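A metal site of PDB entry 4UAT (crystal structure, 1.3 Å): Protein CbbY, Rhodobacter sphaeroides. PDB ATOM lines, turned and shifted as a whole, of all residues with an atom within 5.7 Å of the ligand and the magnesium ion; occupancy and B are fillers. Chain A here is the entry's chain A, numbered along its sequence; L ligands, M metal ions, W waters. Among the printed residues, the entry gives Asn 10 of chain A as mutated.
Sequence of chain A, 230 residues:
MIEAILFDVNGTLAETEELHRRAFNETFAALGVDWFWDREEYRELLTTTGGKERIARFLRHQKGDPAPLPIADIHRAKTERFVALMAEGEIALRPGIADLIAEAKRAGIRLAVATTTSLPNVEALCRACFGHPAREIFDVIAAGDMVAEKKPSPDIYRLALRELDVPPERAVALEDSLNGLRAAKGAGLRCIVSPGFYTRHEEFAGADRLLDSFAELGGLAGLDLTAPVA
Water W2 lies within hydrogen-bond range of OE1 of Glu 175, OG of Ser 177 and OD1 of Asp 8. Water W7 bridges O11 of the ligand and O of Thr 116. Water W3 lies within hydrogen-bond range of the side-chain amino group (NZ) of Lys 78 (2.7 Å), an oxygen (O9) of the ligand (2.7 Å), the side-chain hydroxyl (OG1) of Thr 79 (2.8 Å) and the side-chain amide nitrogen (ND2) of Asn 121 (3.0 Å). Water W4 bridges the backbone carbonyl oxygen (O) of Leu 46 and an oxygen (O2) of the ligand.
Residues that only touch the ligand: His 20 (3.5 Å), Phe 24 (3.9 Å), Tyr 42 (3.9 Å), Leu 46 (3.9 Å) and Thr 49 (3.4 Å). Hydrophobic or aromatic side chains that line the ligand: Val 9, His 20, Phe 24, Leu 46 and His 75.
The backbone NH (N) of Asn 10 sits at hydrogen-bond distance from an oxygen (O6) of the ligand, 2.7 Å away. The side-chain amide nitrogen of Asn 10 sits at hydrogen-bond distance from an oxygen (O1) of the ligand (2.7 Å). O4 of the ligand lies within hydrogen-bond range of OE2 of Glu 17 (2.6 Å). The side-chain hydroxyl (OG1) of Thr 115 lies within hydrogen-bond range of an oxygen (O6) of the ligand, at 2.6 Å. The backbone NH (N) of Ser 118 is in hydrogen-bond range of an oxygen (O9) of the ligand, 2.9 Å away. The side-chain hydroxyl (OG) of Ser 118 lies within hydrogen-bond range of an oxygen (O9) of the ligand, 2.7 Å away. An oxygen (O10) of the ligand sits at hydrogen-bond distance from a ring nitrogen (NE2) of His 75, 2.7 Å away. N of Gly 51 sits at hydrogen-bond distance from O11 of the ligand (2.7 Å). The guanidinium group (NH1) of Arg 54 lies within hydrogen-bond range of an oxygen (O4) of the ligand (2.8 Å). N of Thr 116 sits at hydrogen-bond distance from O8 of the ligand. O8 of the ligand is in hydrogen-bond range of OG1 of Thr 116. The side-chain amino group of Lys 78 lies within salt-bridge range of an oxygen (O10) of the ligand (2.8 Å). N of Gly 50 lies within hydrogen-bond range of O3 of the ligand (2.8 Å). An oxygen (O5) of the ligand is in hydrogen-bond range of the side-chain hydroxyl (OG1) of Thr 117. An oxygen (O9) of the ligand lies within hydrogen-bond range of the side-chain amide nitrogen of Asn 121, at 2.9 Å. N of Val 9 lies within hydrogen-bond range of O6 of the ligand (3.4 Å). NZ of Lys 151 is in salt-bridge range of O8 of the ligand (3.5 Å).
Three residues have an atom within 4 Å of the magnesium ion: Asp 8, Asn 10 and Asp 176.
The magnesium ion is bound by an oxygen (O7) of the ligand (2.0 Å), the side-chain carboxylate of Asp 8 (2.0 Å), the backbone carbonyl oxygen of Asn 10 (2.1 Å), the side-chain carboxylate of Asp 176 (2.1 Å), water W6 (2.1 Å) and water W2 (2.1 Å).
The side-chain carboxylate (OD1) of Asp 8 lies within salt-bridge range of the side-chain amino group (NZ) of Lys 151, at 2.7 Å. The side-chain amide oxygen of Asn 10 is in hydrogen-bond range of a ring nitrogen (NE2) of His 20, at 2.8 Å. The side-chain carboxylate of Glu 17 is in hydrogen-bond range of the side-chain hydroxyl of Tyr 42 (2.7 Å). The side-chain hydroxyl (OH) of Tyr 42 sits at hydrogen-bond distance from the guanidinium group (NH1) of Arg 54 (3.0 Å). O of Thr 48 is in hydrogen-bond range of NH2 of Arg 54 (2.8 Å). The side-chain hydroxyl (OG1) of Thr 49 is in hydrogen-bond range of the backbone carbonyl oxygen (O) of Lys 151, at 2.8 Å. The side-chain carboxylate (OE2) of Glu 175 is in salt-bridge range of the side-chain amino group (NZ) of Lys 151, at 2.8 Å. NZ of Lys 151 lies within hydrogen-bond range of O of Ala 114, at 2.8 Å.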
ATOM      1  N   ASP A   8      18.256 -16.303  32.224  1.00  0.00           N
ATOM      2  CA  ASP A   8      18.509 -16.980  30.976  1.00  0.00           C
ATOM      3  C   ASP A   8      17.183 -17.342  30.316  1.00  0.00           C
ATOM      4  O   ASP A   8      16.130 -17.395  30.967  1.00  0.00           O
ATOM      5  CB  ASP A   8      19.323 -18.219  31.278  1.00  0.00           C
ATOM      6  CG  ASP A   8      19.676 -18.995  30.073  1.00  0.00           C
ATOM      7  OD1 ASP A   8      20.249 -18.375  29.145  1.00  0.00           O
ATOM      8  OD2 ASP A   8      19.361 -20.201  30.007  1.00  0.00           O
ATOM      9  N   VAL A   9      17.207 -17.694  29.037  1.00  0.00           N
ATOM     10  CA  VAL A   9      16.001 -18.101  28.333  1.00  0.00           C
ATOM     11  C   VAL A   9      15.983 -19.623  28.095  1.00  0.00           C
ATOM     12  O   VAL A   9      15.179 -20.326  28.739  1.00  0.00           O
ATOM     13  CB  VAL A   9      15.783 -17.307  27.053  1.00  0.00           C
ATOM     14  CG1 VAL A   9      14.575 -17.862  26.248  1.00  0.00           C
ATOM     15  CG2 VAL A   9      15.560 -15.838  27.399  1.00  0.00           C
ATOM     16  N   ASN A  10      16.815 -20.144  27.190  1.00  0.00           N
ATOM     17  CA  ASN A  10      16.688 -21.521  26.806  1.00  0.00           C
ATOM     18  C   ASN A  10      17.172 -22.453  27.911  1.00  0.00           C
ATOM     19  O   ASN A  10      18.297 -22.360  28.390  1.00  0.00           O
ATOM     20  CB  ASN A  10      17.451 -21.773  25.488  1.00  0.00           C
ATOM     21  CG  ASN A  10      16.886 -20.963  24.361  1.00  0.00           C
ATOM     22  OD1 ASN A  10      15.663 -21.168  24.029  1.00  0.00           O
ATOM     23  ND2 ASN A  10      17.638 -20.097  23.730  1.00  0.00           N
ATOM     24  N   GLY A  11      16.276 -23.372  28.249  1.00  0.00           N
ATOM     25  CA  GLY A  11      16.474 -24.279  29.345  1.00  0.00           C
ATOM     26  C   GLY A  11      16.184 -23.740  30.729  1.00  0.00           C
ATOM     27  O   GLY A  11      16.198 -24.488  31.688  1.00  0.00           O
ATOM     28  N   THR A  12      15.866 -22.455  30.809  1.00  0.00           N
ATOM     29  CA  THR A  12      15.655 -21.747  32.073  1.00  0.00           C
ATOM     30  C   THR A  12      14.189 -21.327  32.194  1.00  0.00           C
ATOM     31  O   THR A  12      13.487 -21.794  33.044  1.00  0.00           O
ATOM     32  CB  THR A  12      16.689 -20.616  32.250  1.00  0.00           C
ATOM     33  OG1 THR A  12      18.017 -21.156  32.282  1.00  0.00           O
ATOM     34  CG2 THR A  12      16.457 -19.839  33.552  1.00  0.00           C
ATOM     35  N   GLU A  17      15.202 -26.675  23.893  1.00  0.00           N
ATOM     36  CA  GLU A  17      16.225 -27.070  22.964  1.00  0.00           C
ATOM     37  C   GLU A  17      15.826 -28.128  21.977  1.00  0.00           C
ATOM     38  O   GLU A  17      16.306 -28.091  20.853  1.00  0.00           O
ATOM     39  CB  GLU A  17      17.546 -27.387  23.631  1.00  0.00           C
ATOM     40  CG  GLU A  17      18.341 -26.149  24.067  1.00  0.00           C
ATOM     41  CD  GLU A  17      18.807 -25.253  22.912  1.00  0.00           C
ATOM     42  OE1 GLU A  17      18.684 -25.657  21.733  1.00  0.00           O
ATOM     43  OE2 GLU A  17      19.384 -24.172  23.247  1.00  0.00           O
ATOM     44  N   HIS A  20      14.318 -26.076  19.309  1.00  0.00           N
ATOM     45  CA  HIS A  20      15.410 -25.516  18.482  1.00  0.00           C
ATOM     46  C   HIS A  20      15.941 -26.572  17.524  1.00  0.00           C
ATOM     47  O   HIS A  20      16.136 -26.264  16.340  1.00  0.00           O
ATOM     48  CB  HIS A  20      16.525 -24.932  19.305  1.00  0.00           C
ATOM     49  CG  HIS A  20      16.165 -23.640  19.974  1.00  0.00           C
ATOM     50  ND1 HIS A  20      16.052 -22.454  19.275  1.00  0.00           N
ATOM     51  CD2 HIS A  20      15.942 -23.344  21.287  1.00  0.00           C
ATOM     52  CE1 HIS A  20      15.783 -21.484  20.138  1.00  0.00           C
ATOM     53  NE2 HIS A  20      15.683 -21.994  21.355  1.00  0.00           N
ATOM     54  N   PHE A  24      16.068 -26.306  13.474  1.00  0.00           N
ATOM     55  CA  PHE A  24      17.281 -26.477  12.662  1.00  0.00           C
ATOM     56  C   PHE A  24      17.060 -27.528  11.579  1.00  0.00           C
ATOM     57  O   PHE A  24      17.273 -27.308  10.418  1.00  0.00           O
ATOM     58  CB  PHE A  24      18.531 -26.765  13.491  1.00  0.00           C
ATOM     59  CG  PHE A  24      19.116 -25.609  14.232  1.00  0.00           C
ATOM     60  CD1 PHE A  24      19.837 -24.606  13.597  1.00  0.00           C
ATOM     61  CD2 PHE A  24      19.088 -25.553  15.601  1.00  0.00           C
ATOM     62  CE1 PHE A  24      20.452 -23.588  14.290  1.00  0.00           C
ATOM     63  CE2 PHE A  24      19.691 -24.528  16.293  1.00  0.00           C
ATOM     64  CZ  PHE A  24      20.377 -23.544  15.643  1.00  0.00           C
ATOM     65  N   TYR A  42      23.758 -32.824  18.596  1.00  0.00           N
ATOM     66  CA  TYR A  42      23.272 -31.534  19.127  1.00  0.00           C
ATOM     67  C   TYR A  42      23.790 -31.267  20.542  1.00  0.00           C
ATOM     68  O   TYR A  42      24.117 -30.133  20.863  1.00  0.00           O
ATOM     69  CB  TYR A  42      21.743 -31.474  19.056  1.00  0.00           C
ATOM     70  CG  TYR A  42      21.185 -30.070  19.163  1.00  0.00           C
ATOM     71  CD1 TYR A  42      21.518 -29.118  18.192  1.00  0.00           C
ATOM     72  CD2 TYR A  42      20.286 -29.665  20.160  1.00  0.00           C
ATOM     73  CE1 TYR A  42      21.002 -27.840  18.224  1.00  0.00           C
ATOM     74  CE2 TYR A  42      19.811 -28.357  20.208  1.00  0.00           C
ATOM     75  CZ  TYR A  42      20.179 -27.446  19.282  1.00  0.00           C
ATOM     76  OH  TYR A  42      19.757 -26.146  19.337  1.00  0.00           O
ATOM     77  N   LEU A  46      25.715 -27.813  21.282  1.00  0.00           N
ATOM     78  CA  LEU A  46      25.170 -26.884  22.258  1.00  0.00           C
ATOM     79  C   LEU A  46      26.222 -26.231  23.122  1.00  0.00           C
ATOM     80  O   LEU A  46      25.908 -25.225  23.798  1.00  0.00           O
ATOM     81  CB  LEU A  46      24.117 -27.556  23.150  1.00  0.00           C
ATOM     82  CG  LEU A  46      22.732 -27.704  22.544  1.00  0.00           C
ATOM     83  CD1 LEU A  46      21.852 -28.647  23.328  1.00  0.00           C
ATOM     84  CD2 LEU A  46      22.033 -26.341  22.399  1.00  0.00           C
ATOM     85  N   THR A  48      28.621 -24.582  21.995  1.00  0.00           N
ATOM     86  CA  THR A  48      28.803 -23.297  21.316  1.00  0.00           C
ATOM     87  C   THR A  48      27.457 -22.564  21.303  1.00  0.00           C
ATOM     88  O   THR A  48      26.509 -23.072  20.716  1.00  0.00           O
ATOM     89  CB  THR A  48      29.246 -23.534  19.883  1.00  0.00           C
ATOM     90  OG1 THR A  48      30.499 -24.226  19.894  1.00  0.00           O
ATOM     91  CG2 THR A  48      29.347 -22.290  19.112  1.00  0.00           C
ATOM     92  N   THR A  49      27.379 -21.421  21.991  1.00  0.00           N
ATOM     93  CA  THR A  49      26.170 -20.686  22.037  1.00  0.00           C
ATOM     94  C   THR A  49      25.994 -19.767  20.833  1.00  0.00           C
ATOM     95  O   THR A  49      26.930 -19.320  20.197  1.00  0.00           O
ATOM     96  CB  THR A  49      26.028 -19.879  23.311  1.00  0.00           C
ATOM     97  OG1 THR A  49      26.954 -18.779  23.270  1.00  0.00           O
ATOM     98  CG2 THR A  49      26.218 -20.752  24.557  1.00  0.00           C
ATOM     99  N   GLY A  50      24.708 -19.565  20.483  1.00  0.00           N
ATOM    100  CA  GLY A  50      24.304 -18.802  19.318  1.00  0.00           C
ATOM    101  C   GLY A  50      24.167 -19.712  18.136  1.00  0.00           C
ATOM    102  O   GLY A  50      25.064 -20.488  17.795  1.00  0.00           O
ATOM    103  N   GLY A  51      23.000 -19.605  17.469  1.00  0.00           N
ATOM    104  CA  GLY A  51      22.739 -20.563  16.371  1.00  0.00           C
ATOM    105  C   GLY A  51      23.630 -20.330  15.163  1.00  0.00           C
ATOM    106  O   GLY A  51      23.972 -21.258  14.441  1.00  0.00           O
ATOM    107  N   LYS A  52      23.948 -19.052  14.856  1.00  0.00           N
ATOM    108  CA  LYS A  52      24.869 -18.787  13.753  1.00  0.00           C
ATOM    109  C   LYS A  52      26.230 -19.394  14.032  1.00  0.00           C
ATOM    110  O   LYS A  52      26.869 -20.032  13.150  1.00  0.00           O
ATOM    111  CB  LYS A  52      24.986 -17.288  13.470  1.00  0.00           C
ATOM    112  CG  LYS A  52      23.693 -16.703  12.958  1.00  0.00           C
ATOM    113  CD  LYS A  52      23.842 -15.223  12.487  1.00  0.00           C
ATOM    114  CE  LYS A  52      24.187 -14.276  13.597  1.00  0.00           C
ATOM    115  NZ  LYS A  52      23.231 -14.210  14.686  1.00  0.00           N
ATOM    116  N   ARG A  54      26.861 -21.826  16.052  1.00  0.00           N
ATOM    117  CA  ARG A  54      26.744 -23.260  16.073  1.00  0.00           C
ATOM    118  C   ARG A  54      26.816 -23.811  14.638  1.00  0.00           C
ATOM    119  O   ARG A  54      27.491 -24.791  14.377  1.00  0.00           O
ATOM    120  CB  ARG A  54      25.429 -23.681  16.778  1.00  0.00           C
ATOM    121  CG  ARG A  54      25.278 -25.169  16.986  1.00  0.00           C
ATOM    122  CD  ARG A  54      24.045 -25.504  17.844  1.00  0.00           C
ATOM    123  NE  ARG A  54      24.201 -24.895  19.109  1.00  0.00           N
ATOM    124  CZ  ARG A  54      23.330 -24.105  19.686  1.00  0.00           C
ATOM    125  NH1 ARG A  54      22.036 -24.141  19.355  1.00  0.00           N
ATOM    126  NH2 ARG A  54      23.712 -23.318  20.660  1.00  0.00           N
ATOM    127  N   HIS A  75      20.110 -19.135   9.265  1.00  0.00           N
ATOM    128  CA  HIS A  75      19.676 -18.939  10.629  1.00  0.00           C
ATOM    129  C   HIS A  75      18.324 -18.134  10.685  1.00  0.00           C
ATOM    130  O   HIS A  75      17.514 -18.380  11.561  1.00  0.00           O
ATOM    131  CB  HIS A  75      20.769 -18.318  11.468  1.00  0.00           C
ATOM    132  CG  HIS A  75      20.388 -18.301  12.910  1.00  0.00           C
ATOM    133  ND1 HIS A  75      19.963 -17.210  13.570  1.00  0.00           N
ATOM    134  CD2 HIS A  75      20.333 -19.335  13.808  1.00  0.00           C
ATOM    135  CE1 HIS A  75      19.659 -17.531  14.809  1.00  0.00           C
ATOM    136  NE2 HIS A  75      19.878 -18.800  14.968  1.00  0.00           N
ATOM    137  N   LYS A  78      15.621 -20.521  10.123  1.00  0.00           N
ATOM    138  CA  LYS A  78      15.439 -21.319  11.307  1.00  0.00           C
ATOM    139  C   LYS A  78      14.669 -20.552  12.393  1.00  0.00           C
ATOM    140  O   LYS A  78      13.863 -21.152  13.098  1.00  0.00           O
ATOM    141  CB  LYS A  78      16.795 -21.809  11.797  1.00  0.00           C
ATOM    142  CG  LYS A  78      16.751 -22.538  13.142  1.00  0.00           C
ATOM    143  CD  LYS A  78      16.997 -21.663  14.340  1.00  0.00           C
ATOM    144  CE  LYS A  78      16.747 -22.340  15.656  1.00  0.00           C
ATOM    145  NZ  LYS A  78      16.959 -21.423  16.808  1.00  0.00           N
ATOM    146  N   THR A  79      15.003 -19.257  12.543  1.00  0.00           N
ATOM    147  CA  THR A  79      14.309 -18.454  13.539  1.00  0.00           C
ATOM    148  C   THR A  79      12.828 -18.318  13.213  1.00  0.00           C
ATOM    149  O   THR A  79      11.965 -18.432  14.092  1.00  0.00           O
ATOM    150  CB  THR A  79      14.986 -17.110  13.676  1.00  0.00           C
ATOM    151  OG1 THR A  79      16.343 -17.271  14.117  1.00  0.00           O
ATOM    152  CG2 THR A  79      14.279 -16.188  14.640  1.00  0.00           C
ATOM    153  N   ALA A 114      18.805 -12.257  29.917  1.00  0.00           N
ATOM    154  CA  ALA A 114      20.195 -12.244  29.453  1.00  0.00           C
ATOM    155  C   ALA A 114      20.462 -13.569  28.761  1.00  0.00           C
ATOM    156  O   ALA A 114      20.596 -14.596  29.413  1.00  0.00           O
ATOM    157  CB  ALA A 114      21.169 -12.032  30.589  1.00  0.00           C
ATOM    158  N   THR A 115      20.436 -13.544  27.414  1.00  0.00           N
ATOM    159  CA  THR A 115      20.359 -14.738  26.593  1.00  0.00           C
ATOM    160  C   THR A 115      21.285 -14.628  25.420  1.00  0.00           C
ATOM    161  O   THR A 115      21.468 -13.585  24.852  1.00  0.00           O
ATOM    162  CB  THR A 115      18.895 -15.043  26.157  1.00  0.00           C
ATOM    163  OG1 THR A 115      18.866 -16.235  25.353  1.00  0.00           O
ATOM    164  CG2 THR A 115      18.304 -13.941  25.381  1.00  0.00           C
ATOM    165  N   THR A 116      21.726 -15.813  24.953  1.00  0.00           N
ATOM    166  CA  THR A 116      22.404 -15.950  23.674  1.00  0.00           C
ATOM    167  C   THR A 116      21.448 -15.994  22.492  1.00  0.00           C
ATOM    168  O   THR A 116      21.920 -15.867  21.346  1.00  0.00           O
ATOM    169  CB  THR A 116      23.319 -17.174  23.668  1.00  0.00           C
ATOM    170  OG1 THR A 116      22.556 -18.360  23.660  1.00  0.00           O
ATOM    171  CG2 THR A 116      24.306 -17.113  24.824  1.00  0.00           C
ATOM    172  N   THR A 117      20.162 -16.217  22.726  1.00  0.00           N
ATOM    173  CA  THR A 117      19.220 -16.541  21.696  1.00  0.00           C
ATOM    174  C   THR A 117      18.757 -15.285  20.938  1.00  0.00           C
ATOM    175  O   THR A 117      18.848 -14.170  21.428  1.00  0.00           O
ATOM    176  CB  THR A 117      18.011 -17.268  22.314  1.00  0.00           C
ATOM    177  OG1 THR A 117      17.433 -18.223  21.394  1.00  0.00           O
ATOM    178  CG2 THR A 117      16.873 -16.400  22.814  1.00  0.00           C
ATOM    179  N   SER A 118      18.229 -15.517  19.764  1.00  0.00           N
ATOM    180  CA  SER A 118      17.718 -14.430  18.887  1.00  0.00           C
ATOM    181  C   SER A 118      16.542 -13.720  19.554  1.00  0.00           C
ATOM    182  O   SER A 118      15.675 -14.378  20.128  1.00  0.00           O
ATOM    183  CB  SER A 118      17.298 -14.990  17.576  1.00  0.00           C
ATOM    184  OG  SER A 118      18.369 -15.702  16.986  1.00  0.00           O
ATOM    185  N   ASN A 121      12.909 -15.001  19.309  1.00  0.00           N
ATOM    186  CA  ASN A 121      12.567 -16.144  20.147  1.00  0.00           C
ATOM    187  C   ASN A 121      12.066 -15.758  21.512  1.00  0.00           C
ATOM    188  O   ASN A 121      11.209 -16.414  22.088  1.00  0.00           O
ATOM    189  CB  ASN A 121      13.769 -17.060  20.312  1.00  0.00           C
ATOM    190  CG  ASN A 121      14.358 -17.588  19.000  1.00  0.00           C
ATOM    191  OD1 ASN A 121      13.705 -17.598  17.970  1.00  0.00           O
ATOM    192  ND2 ASN A 121      15.604 -18.043  19.101  1.00  0.00           N
ATOM    193  N   LYS A 150      29.372 -14.124  22.879  1.00  0.00           N
ATOM    194  CA  LYS A 150      28.336 -14.798  23.582  1.00  0.00           C
ATOM    195  C   LYS A 150      28.818 -15.636  24.758  1.00  0.00           C
ATOM    196  O   LYS A 150      30.010 -15.833  24.953  1.00  0.00           O
ATOM    197  CB  LYS A 150      27.470 -15.647  22.612  1.00  0.00           C
ATOM    198  CG  LYS A 150      26.688 -14.833  21.616  1.00  0.00           C
ATOM    199  CD  LYS A 150      25.860 -15.641  20.682  1.00  0.00           C
ATOM    200  CE  LYS A 150      24.909 -14.884  19.804  1.00  0.00           C
ATOM    201  NZ  LYS A 150      25.599 -14.086  18.771  1.00  0.00           N
ATOM    202  N   LYS A 151      27.923 -16.035  25.612  1.00  0.00           N
ATOM    203  CA  LYS A 151      28.259 -16.888  26.747  1.00  0.00           C
ATOM    204  C   LYS A 151      29.156 -18.018  26.263  1.00  0.00           C
ATOM    205  O   LYS A 151      28.862 -18.631  25.252  1.00  0.00           O
ATOM    206  CB  LYS A 151      26.979 -17.425  27.396  1.00  0.00           C
ATOM    207  CG  LYS A 151      25.983 -16.360  27.876  1.00  0.00           C
ATOM    208  CD  LYS A 151      24.785 -16.978  28.596  1.00  0.00           C
ATOM    209  CE  LYS A 151      23.573 -16.066  28.733  1.00  0.00           C
ATOM    210  NZ  LYS A 151      22.390 -16.781  29.213  1.00  0.00           N
ATOM    211  N   GLU A 175      20.047 -19.756  35.636  1.00  0.00           N
ATOM    212  CA  GLU A 175      20.665 -20.397  34.458  1.00  0.00           C
ATOM    213  C   GLU A 175      20.422 -21.861  34.472  1.00  0.00           C
ATOM    214  O   GLU A 175      20.062 -22.470  35.491  1.00  0.00           O
ATOM    215  CB  GLU A 175      22.201 -20.137  34.531  1.00  0.00           C
ATOM    216  CG  GLU A 175      22.588 -18.813  33.881  1.00  0.00           C
ATOM    217  CD  GLU A 175      22.521 -18.833  32.387  1.00  0.00           C
ATOM    218  OE1 GLU A 175      22.236 -19.923  31.830  1.00  0.00           O
ATOM    219  OE2 GLU A 175      22.851 -17.799  31.749  1.00  0.00           O
ATOM    220  N   ASP A 176      20.710 -22.496  33.339  1.00  0.00           N
ATOM    221  CA  ASP A 176      20.581 -23.939  33.167  1.00  0.00           C
ATOM    222  C   ASP A 176      21.862 -24.640  32.697  1.00  0.00           C
ATOM    223  O   ASP A 176      21.897 -25.863  32.750  1.00  0.00           O
ATOM    224  CB  ASP A 176      19.484 -24.290  32.115  1.00  0.00           C
ATOM    225  CG  ASP A 176      19.943 -23.907  30.695  1.00  0.00           C
ATOM    226  OD1 ASP A 176      20.236 -22.724  30.507  1.00  0.00           O
ATOM    227  OD2 ASP A 176      19.947 -24.816  29.836  1.00  0.00           O
ATOM    228  N   SER A 177      22.854 -23.867  32.220  1.00  0.00           N
ATOM    229  CA  SER A 177      23.974 -24.448  31.506  1.00  0.00           C
ATOM    230  C   SER A 177      25.314 -23.952  32.057  1.00  0.00           C
ATOM    231  O   SER A 177      25.338 -22.900  32.689  1.00  0.00           O
ATOM    232  CB  SER A 177      23.927 -24.114  30.006  1.00  0.00           C
ATOM    233  OG  SER A 177      24.241 -22.754  29.740  1.00  0.00           O
HETATM  234  C1  LIG L   1      21.182 -21.058  24.291  1.00  0.00           C
HETATM  235  C2  LIG L   1      21.791 -20.997  22.942  1.00  0.00           C
HETATM  236  C3  LIG L   1      21.061 -20.496  21.741  1.00  0.00           C
HETATM  237  C4  LIG L   1      19.989 -21.529  21.378  1.00  0.00           C
HETATM  238  C5  LIG L   1      19.393 -21.341  19.973  1.00  0.00           C
HETATM  239  O1  LIG L   1      20.224 -19.895  24.635  1.00  0.00           O
HETATM  240  O2  LIG L   1      22.968 -21.394  22.772  1.00  0.00           O
HETATM  241  O3  LIG L   1      21.967 -20.275  20.666  1.00  0.00           O
HETATM  242  O4  LIG L   1      20.567 -22.863  21.375  1.00  0.00           O
HETATM  243  O5  LIG L   1      18.912 -20.022  19.748  1.00  0.00           O
HETATM  244  P1  LIG L   1      20.271 -19.249  26.238  1.00  0.00           P
HETATM  245  P2  LIG L   1      19.424 -19.160  18.468  1.00  0.00           P
HETATM  246  O6  LIG L   1      18.926 -18.638  26.285  1.00  0.00           O
HETATM  247  O7  LIG L   1      20.344 -20.502  27.043  1.00  0.00           O
HETATM  248  O8  LIG L   1      21.489 -18.418  26.278  1.00  0.00           O
HETATM  249  O9  LIG L   1      18.437 -18.039  18.344  1.00  0.00           O
HETATM  250  O10 LIG L   1      19.418 -20.101  17.294  1.00  0.00           O
HETATM  251  O11 LIG L   1      20.805 -18.681  18.832  1.00  0.00           O
HETATM  252 MG    MG M   1      20.194 -21.523  28.757  1.00  0.00          MG
HETATM  253  O   HOH W   1      20.946 -24.367  25.402  1.00  0.00           O
HETATM  254  O   HOH W   2      22.165 -20.971  29.375  1.00  0.00           O
HETATM  255  O   HOH W   3      16.685 -18.786  16.413  1.00  0.00           O
HETATM  256  O   HOH W   4      23.723 -23.665  24.376  1.00  0.00           O
HETATM  257  O   HOH W   5      23.577 -19.838  27.352  1.00  0.00           O
HETATM  258  O   HOH W   6      21.044 -23.253  27.851  1.00  0.00           O
HETATM  259  O   HOH W   7      21.744 -16.186  18.615  1.00  0.00           O
